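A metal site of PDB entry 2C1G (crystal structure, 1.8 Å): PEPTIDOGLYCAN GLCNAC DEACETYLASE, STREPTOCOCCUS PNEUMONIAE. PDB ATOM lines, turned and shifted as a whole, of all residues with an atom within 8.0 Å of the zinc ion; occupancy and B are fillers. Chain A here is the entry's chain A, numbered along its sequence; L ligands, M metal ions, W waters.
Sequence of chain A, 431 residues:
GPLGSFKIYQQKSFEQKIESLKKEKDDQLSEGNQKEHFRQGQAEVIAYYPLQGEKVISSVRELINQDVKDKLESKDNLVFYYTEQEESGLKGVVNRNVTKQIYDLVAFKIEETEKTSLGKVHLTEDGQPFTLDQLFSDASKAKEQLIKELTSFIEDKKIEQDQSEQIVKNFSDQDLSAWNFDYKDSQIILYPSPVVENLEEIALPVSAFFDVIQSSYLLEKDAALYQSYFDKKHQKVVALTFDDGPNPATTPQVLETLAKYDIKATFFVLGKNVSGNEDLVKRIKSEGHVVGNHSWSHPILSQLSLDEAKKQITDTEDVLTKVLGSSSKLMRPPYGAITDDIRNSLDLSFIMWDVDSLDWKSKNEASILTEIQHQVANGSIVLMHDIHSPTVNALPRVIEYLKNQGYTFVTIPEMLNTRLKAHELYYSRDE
N of Asp 244 lies within hydrogen-bond range of O of Phe 268, at 3.2 Å.
ND1 of His 298 lies within hydrogen-bond range of OH of Tyr 335, 3.1 Å away.
The side-chain hydroxyl (OG) of Ser 295 sits at hydrogen-bond distance from the backbone NH (N) of His 298.
A ring nitrogen (ND1) of His 294 sits at hydrogen-bond distance from the backbone carbonyl oxygen (O) of Arg 332, at 2.7 Å.
NH1 of Arg 332 lies within salt-bridge range of OD1 of Asp 243, 2.9 Å away.
O of Met 384 is in hydrogen-bond range of N of Asp 243 (2.9 Å).
Asp 243 touches the zinc ion (CB to ZN, 3.99 Å).
Of the 20 residues printed, 4 come within 4 Å of the zinc ion.
Along chain A the residues within 4 Å of the zinc ion span positions 243 to 298.
The zinc ion is bound by OD1 of Asp 244 (2.0 Å).
NE2 of His 298 binds the zinc ion (2.0 Å).
Water W1 binds the zinc ion.
The zinc ion is bound by a ring nitrogen (NE2) of His 294 (2.2 Å).
An oxygen (O2) of the ligand is bound to the zinc ion (2.3 Å).
The zinc ion is bound by O1 of the ligand.
Water W1 bridges OD2 of Asp 244 (2.6 Å) and NE2 of His 385 (3.2 Å).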
ATOM      1  N   PHE A 242      26.472 -12.217 -22.022  1.00  0.00           N
ATOM      2  CA  PHE A 242      27.614 -13.121 -22.036  1.00  0.00           C
ATOM      3  C   PHE A 242      28.203 -13.215 -20.662  1.00  0.00           C
ATOM      4  O   PHE A 242      28.577 -12.202 -20.071  1.00  0.00           O
ATOM      5  CB  PHE A 242      28.675 -12.578 -22.981  1.00  0.00           C
ATOM      6  CG  PHE A 242      28.239 -12.544 -24.423  1.00  0.00           C
ATOM      7  CD1 PHE A 242      28.288 -13.700 -25.205  1.00  0.00           C
ATOM      8  CD2 PHE A 242      27.753 -11.366 -24.980  1.00  0.00           C
ATOM      9  CE1 PHE A 242      27.850 -13.669 -26.543  1.00  0.00           C
ATOM     10  CE2 PHE A 242      27.304 -11.336 -26.320  1.00  0.00           C
ATOM     11  CZ  PHE A 242      27.351 -12.494 -27.093  1.00  0.00           C
ATOM     12  N   ASP A 243      28.318 -14.441 -20.174  1.00  0.00           N
ATOM     13  CA  ASP A 243      28.843 -14.712 -18.828  1.00  0.00           C
ATOM     14  C   ASP A 243      30.253 -15.304 -18.801  1.00  0.00           C
ATOM     15  O   ASP A 243      30.699 -15.958 -19.761  1.00  0.00           O
ATOM     16  CB  ASP A 243      27.947 -15.752 -18.103  1.00  0.00           C
ATOM     17  CG  ASP A 243      26.605 -15.201 -17.652  1.00  0.00           C
ATOM     18  OD1 ASP A 243      26.286 -14.034 -17.945  1.00  0.00           O
ATOM     19  OD2 ASP A 243      25.848 -15.963 -16.985  1.00  0.00           O
ATOM     20  N   ASP A 244      30.868 -15.122 -17.624  1.00  0.00           N
ATOM     21  CA  ASP A 244      32.150 -15.694 -17.218  1.00  0.00           C
ATOM     22  C   ASP A 244      33.443 -15.063 -17.712  1.00  0.00           C
ATOM     23  O   ASP A 244      34.524 -15.566 -17.394  1.00  0.00           O
ATOM     24  CB  ASP A 244      32.211 -17.203 -17.541  1.00  0.00           C
ATOM     25  CG  ASP A 244      31.115 -18.052 -16.852  1.00  0.00           C
ATOM     26  OD1 ASP A 244      30.169 -17.580 -16.169  1.00  0.00           O
ATOM     27  OD2 ASP A 244      31.199 -19.291 -16.995  1.00  0.00           O
ATOM     28  N   GLY A 245      33.339 -13.987 -18.479  1.00  0.00           N
ATOM     29  CA  GLY A 245      34.541 -13.355 -18.982  1.00  0.00           C
ATOM     30  C   GLY A 245      35.111 -12.318 -18.037  1.00  0.00           C
ATOM     31  O   GLY A 245      34.768 -12.272 -16.854  1.00  0.00           O
ATOM     32  N   PHE A 268      28.326 -10.142 -18.213  1.00  0.00           N
ATOM     33  CA  PHE A 268      28.362 -10.360 -16.765  1.00  0.00           C
ATOM     34  C   PHE A 268      29.716 -11.021 -16.515  1.00  0.00           C
ATOM     35  O   PHE A 268      29.911 -12.215 -16.750  1.00  0.00           O
ATOM     36  CB  PHE A 268      27.182 -11.232 -16.331  1.00  0.00           C
ATOM     37  CG  PHE A 268      25.859 -10.501 -16.377  1.00  0.00           C
ATOM     38  CD1 PHE A 268      25.499  -9.622 -15.363  1.00  0.00           C
ATOM     39  CD2 PHE A 268      24.997 -10.638 -17.478  1.00  0.00           C
ATOM     40  CE1 PHE A 268      24.315  -8.889 -15.433  1.00  0.00           C
ATOM     41  CE2 PHE A 268      23.806  -9.903 -17.559  1.00  0.00           C
ATOM     42  CZ  PHE A 268      23.455  -9.024 -16.543  1.00  0.00           C
ATOM     43  N   LEU A 270      33.326 -12.018 -14.330  1.00  0.00           N
ATOM     44  CA  LEU A 270      33.786 -12.522 -13.036  1.00  0.00           C
ATOM     45  C   LEU A 270      34.868 -11.574 -12.513  1.00  0.00           C
ATOM     46  O   LEU A 270      35.810 -11.221 -13.236  1.00  0.00           O
ATOM     47  CB  LEU A 270      34.364 -13.940 -13.174  1.00  0.00           C
ATOM     48  CG  LEU A 270      33.316 -15.059 -13.345  1.00  0.00           C
ATOM     49  CD1 LEU A 270      33.992 -16.358 -13.811  1.00  0.00           C
ATOM     50  CD2 LEU A 270      32.579 -15.268 -12.025  1.00  0.00           C
ATOM     51  N   HIS A 294      29.106 -10.869 -12.189  1.00  0.00           N
ATOM     52  CA  HIS A 294      28.799 -12.316 -12.173  1.00  0.00           C
ATOM     53  C   HIS A 294      29.455 -13.015 -10.961  1.00  0.00           C
ATOM     54  O   HIS A 294      29.629 -14.233 -10.965  1.00  0.00           O
ATOM     55  CB  HIS A 294      29.303 -12.953 -13.485  1.00  0.00           C
ATOM     56  CG  HIS A 294      28.697 -14.303 -13.769  1.00  0.00           C
ATOM     57  ND1 HIS A 294      27.395 -14.623 -13.461  1.00  0.00           N
ATOM     58  CD2 HIS A 294      29.222 -15.406 -14.354  1.00  0.00           C
ATOM     59  CE1 HIS A 294      27.142 -15.869 -13.834  1.00  0.00           C
ATOM     60  NE2 HIS A 294      28.234 -16.355 -14.384  1.00  0.00           N
ATOM     61  N   SER A 295      29.754 -12.215  -9.934  1.00  0.00           N
ATOM     62  CA  SER A 295      30.418 -12.639  -8.703  1.00  0.00           C
ATOM     63  C   SER A 295      31.916 -12.592  -8.936  1.00  0.00           C
ATOM     64  O   SER A 295      32.385 -12.320 -10.043  1.00  0.00           O
ATOM     65  CB  SER A 295      30.005 -14.060  -8.228  1.00  0.00           C
ATOM     66  OG  SER A 295      30.700 -15.090  -8.906  1.00  0.00           O
ATOM     67  N   HIS A 298      32.719 -17.229  -9.118  1.00  0.00           N
ATOM     68  CA  HIS A 298      31.718 -18.190  -9.586  1.00  0.00           C
ATOM     69  C   HIS A 298      31.268 -19.304  -8.629  1.00  0.00           C
ATOM     70  O   HIS A 298      31.006 -20.427  -9.046  1.00  0.00           O
ATOM     71  CB  HIS A 298      32.204 -18.761 -10.927  1.00  0.00           C
ATOM     72  CG  HIS A 298      31.090 -19.071 -11.904  1.00  0.00           C
ATOM     73  ND1 HIS A 298      30.318 -20.213 -11.832  1.00  0.00           N
ATOM     74  CD2 HIS A 298      30.610 -18.348 -12.946  1.00  0.00           C
ATOM     75  CE1 HIS A 298      29.414 -20.190 -12.795  1.00  0.00           C
ATOM     76  NE2 HIS A 298      29.568 -19.071 -13.487  1.00  0.00           N
ATOM     77  N   ARG A 332      24.290 -10.963 -12.083  1.00  0.00           N
ATOM     78  CA  ARG A 332      23.762 -12.262 -12.455  1.00  0.00           C
ATOM     79  C   ARG A 332      24.412 -13.355 -11.599  1.00  0.00           C
ATOM     80  O   ARG A 332      25.616 -13.575 -11.678  1.00  0.00           O
ATOM     81  CB  ARG A 332      24.042 -12.605 -13.907  1.00  0.00           C
ATOM     82  CG  ARG A 332      23.565 -14.022 -14.192  1.00  0.00           C
ATOM     83  CD  ARG A 332      23.547 -14.313 -15.661  1.00  0.00           C
ATOM     84  NE  ARG A 332      22.437 -13.621 -16.317  1.00  0.00           N
ATOM     85  CZ  ARG A 332      22.429 -13.392 -17.618  1.00  0.00           C
ATOM     86  NH1 ARG A 332      23.461 -13.794 -18.338  1.00  0.00           N
ATOM     87  NH2 ARG A 332      21.397 -12.794 -18.186  1.00  0.00           N
ATOM     88  N   PRO A 333      23.624 -14.044 -10.772  1.00  0.00           N
ATOM     89  CA  PRO A 333      24.155 -15.103  -9.901  1.00  0.00           C
ATOM     90  C   PRO A 333      24.666 -16.300 -10.671  1.00  0.00           C
ATOM     91  O   PRO A 333      24.028 -16.766 -11.619  1.00  0.00           O
ATOM     92  CB  PRO A 333      22.934 -15.517  -9.062  1.00  0.00           C
ATOM     93  CG  PRO A 333      22.126 -14.253  -9.000  1.00  0.00           C
ATOM     94  CD  PRO A 333      22.230 -13.733 -10.425  1.00  0.00           C
ATOM     95  N   PRO A 334      25.845 -16.818 -10.283  1.00  0.00           N
ATOM     96  CA  PRO A 334      26.369 -18.001 -10.973  1.00  0.00           C
ATOM     97  C   PRO A 334      25.276 -19.075 -10.825  1.00  0.00           C
ATOM     98  O   PRO A 334      24.683 -19.197  -9.758  1.00  0.00           O
ATOM     99  CB  PRO A 334      27.602 -18.344 -10.150  1.00  0.00           C
ATOM    100  CG  PRO A 334      28.142 -16.964  -9.808  1.00  0.00           C
ATOM    101  CD  PRO A 334      26.889 -16.172  -9.456  1.00  0.00           C
ATOM    102  N   TYR A 335      25.017 -19.827 -11.905  1.00  0.00           N
ATOM    103  CA  TYR A 335      24.031 -20.916 -11.949  1.00  0.00           C
ATOM    104  C   TYR A 335      22.614 -20.466 -11.635  1.00  0.00           C
ATOM    105  O   TYR A 335      21.724 -21.286 -11.453  1.00  0.00           O
ATOM    106  CB  TYR A 335      24.414 -22.031 -10.955  1.00  0.00           C
ATOM    107  CG  TYR A 335      25.888 -22.391 -10.960  1.00  0.00           C
ATOM    108  CD1 TYR A 335      26.451 -23.114 -12.008  1.00  0.00           C
ATOM    109  CD2 TYR A 335      26.726 -21.951  -9.934  1.00  0.00           C
ATOM    110  CE1 TYR A 335      27.823 -23.399 -12.037  1.00  0.00           C
ATOM    111  CE2 TYR A 335      28.085 -22.217  -9.960  1.00  0.00           C
ATOM    112  CZ  TYR A 335      28.626 -22.934 -11.001  1.00  0.00           C
ATOM    113  OH  TYR A 335      29.981 -23.161 -11.018  1.00  0.00           O
ATOM    114  N   GLY A 336      22.408 -19.163 -11.564  1.00  0.00           N
ATOM    115  CA  GLY A 336      21.097 -18.652 -11.233  1.00  0.00           C
ATOM    116  C   GLY A 336      20.736 -18.918  -9.786  1.00  0.00           C
ATOM    117  O   GLY A 336      19.569 -18.821  -9.426  1.00  0.00           O
ATOM    118  N   TRP A 353      17.580 -15.024 -16.735  1.00  0.00           N
ATOM    119  CA  TRP A 353      17.406 -15.172 -18.190  1.00  0.00           C
ATOM    120  C   TRP A 353      16.187 -16.065 -18.443  1.00  0.00           C
ATOM    121  O   TRP A 353      15.671 -16.692 -17.522  1.00  0.00           O
ATOM    122  CB  TRP A 353      18.666 -15.820 -18.799  1.00  0.00           C
ATOM    123  CG  TRP A 353      18.954 -17.215 -18.255  1.00  0.00           C
ATOM    124  CD1 TRP A 353      18.441 -18.408 -18.722  1.00  0.00           C
ATOM    125  CD2 TRP A 353      19.731 -17.547 -17.093  1.00  0.00           C
ATOM    126  NE1 TRP A 353      18.842 -19.447 -17.915  1.00  0.00           N
ATOM    127  CE2 TRP A 353      19.638 -18.956 -16.906  1.00  0.00           C
ATOM    128  CE3 TRP A 353      20.494 -16.797 -16.192  1.00  0.00           C
ATOM    129  CZ2 TRP A 353      20.276 -19.609 -15.855  1.00  0.00           C
ATOM    130  CZ3 TRP A 353      21.130 -17.453 -15.132  1.00  0.00           C
ATOM    131  CH2 TRP A 353      21.014 -18.856 -14.980  1.00  0.00           C
ATOM    132  N   TRP A 360      27.266 -23.585 -23.222  1.00  0.00           N
ATOM    133  CA  TRP A 360      28.176 -24.153 -22.219  1.00  0.00           C
ATOM    134  C   TRP A 360      28.122 -25.670 -22.168  1.00  0.00           C
ATOM    135  O   TRP A 360      29.047 -26.307 -21.664  1.00  0.00           O
ATOM    136  CB  TRP A 360      27.844 -23.630 -20.816  1.00  0.00           C
ATOM    137  CG  TRP A 360      26.402 -23.887 -20.362  1.00  0.00           C
ATOM    138  CD1 TRP A 360      25.315 -23.092 -20.606  1.00  0.00           C
ATOM    139  CD2 TRP A 360      25.917 -25.008 -19.614  1.00  0.00           C
ATOM    140  NE1 TRP A 360      24.178 -23.647 -20.049  1.00  0.00           N
ATOM    141  CE2 TRP A 360      24.520 -24.833 -19.440  1.00  0.00           C
ATOM    142  CE3 TRP A 360      26.520 -26.156 -19.077  1.00  0.00           C
ATOM    143  CZ2 TRP A 360      23.716 -25.751 -18.749  1.00  0.00           C
ATOM    144  CZ3 TRP A 360      25.715 -27.074 -18.386  1.00  0.00           C
ATOM    145  CH2 TRP A 360      24.330 -26.862 -18.232  1.00  0.00           C
ATOM    146  N   LEU A 383      21.047 -16.254 -22.469  1.00  0.00           N
ATOM    147  CA  LEU A 383      22.282 -16.619 -21.777  1.00  0.00           C
ATOM    148  C   LEU A 383      23.297 -17.285 -22.706  1.00  0.00           C
ATOM    149  O   LEU A 383      23.006 -18.353 -23.284  1.00  0.00           O
ATOM    150  CB  LEU A 383      21.969 -17.578 -20.615  1.00  0.00           C
ATOM    151  CG  LEU A 383      23.181 -18.324 -19.984  1.00  0.00           C
ATOM    152  CD1 LEU A 383      24.152 -17.333 -19.346  1.00  0.00           C
ATOM    153  CD2 LEU A 383      22.662 -19.309 -18.945  1.00  0.00           C
ATOM    154  N   MET A 384      24.443 -16.654 -22.872  1.00  0.00           N
ATOM    155  CA  MET A 384      25.586 -17.188 -23.634  1.00  0.00           C
ATOM    156  C   MET A 384      26.873 -16.969 -22.803  1.00  0.00           C
ATOM    157  O   MET A 384      26.841 -16.315 -21.766  1.00  0.00           O
ATOM    158  CB  MET A 384      25.736 -16.502 -24.996  1.00  0.00           C
ATOM    159  CG  MET A 384      24.488 -16.664 -25.878  1.00  0.00           C
ATOM    160  SD  MET A 384      24.780 -16.004 -27.544  1.00  0.00           S
ATOM    161  CE  MET A 384      24.143 -14.324 -27.361  1.00  0.00           C
ATOM    162  N   HIS A 385      27.984 -17.521 -23.281  1.00  0.00           N
ATOM    163  CA  HIS A 385      29.286 -17.384 -22.626  1.00  0.00           C
ATOM    164  C   HIS A 385      30.316 -16.956 -23.670  1.00  0.00           C
ATOM    165  O   HIS A 385      30.516 -17.641 -24.668  1.00  0.00           O
ATOM    166  CB  HIS A 385      29.701 -18.726 -22.020  1.00  0.00           C
ATOM    167  CG  HIS A 385      28.771 -19.210 -20.948  1.00  0.00           C
ATOM    168  ND1 HIS A 385      27.545 -19.768 -21.222  1.00  0.00           N
ATOM    169  CD2 HIS A 385      28.883 -19.169 -19.597  1.00  0.00           C
ATOM    170  CE1 HIS A 385      26.923 -20.025 -20.081  1.00  0.00           C
ATOM    171  NE2 HIS A 385      27.713 -19.675 -19.088  1.00  0.00           N
ATOM    172  N   ILE A 387      33.451 -17.086 -23.500  1.00  0.00           N
ATOM    173  CA  ILE A 387      34.758 -17.616 -23.173  1.00  0.00           C
ATOM    174  C   ILE A 387      35.222 -18.848 -23.951  1.00  0.00           C
ATOM    175  O   ILE A 387      36.360 -19.271 -23.769  1.00  0.00           O
ATOM    176  CB  ILE A 387      34.866 -17.892 -21.662  1.00  0.00           C
ATOM    177  CG1 ILE A 387      33.868 -18.965 -21.251  1.00  0.00           C
ATOM    178  CG2 ILE A 387      34.591 -16.588 -20.878  1.00  0.00           C
ATOM    179  CD1 ILE A 387      34.096 -19.494 -19.833  1.00  0.00           C
HETATM  180  C1  LIG L   1      25.960 -18.672 -15.277  1.00  0.00           C
HETATM  181  O1  LIG L   1      26.531 -19.151 -14.301  1.00  0.00           O
HETATM  182  O2  LIG L   1      26.624 -18.276 -16.238  1.00  0.00           O
HETATM  183  C2  LIG L   1      24.436 -18.561 -15.294  1.00  0.00           C
HETATM  184 ZN    ZN M   1      28.607 -18.338 -15.132  1.00  0.00          ZN
HETATM  185  O   HOH W   1      28.887 -20.134 -16.200  1.00  0.00           O
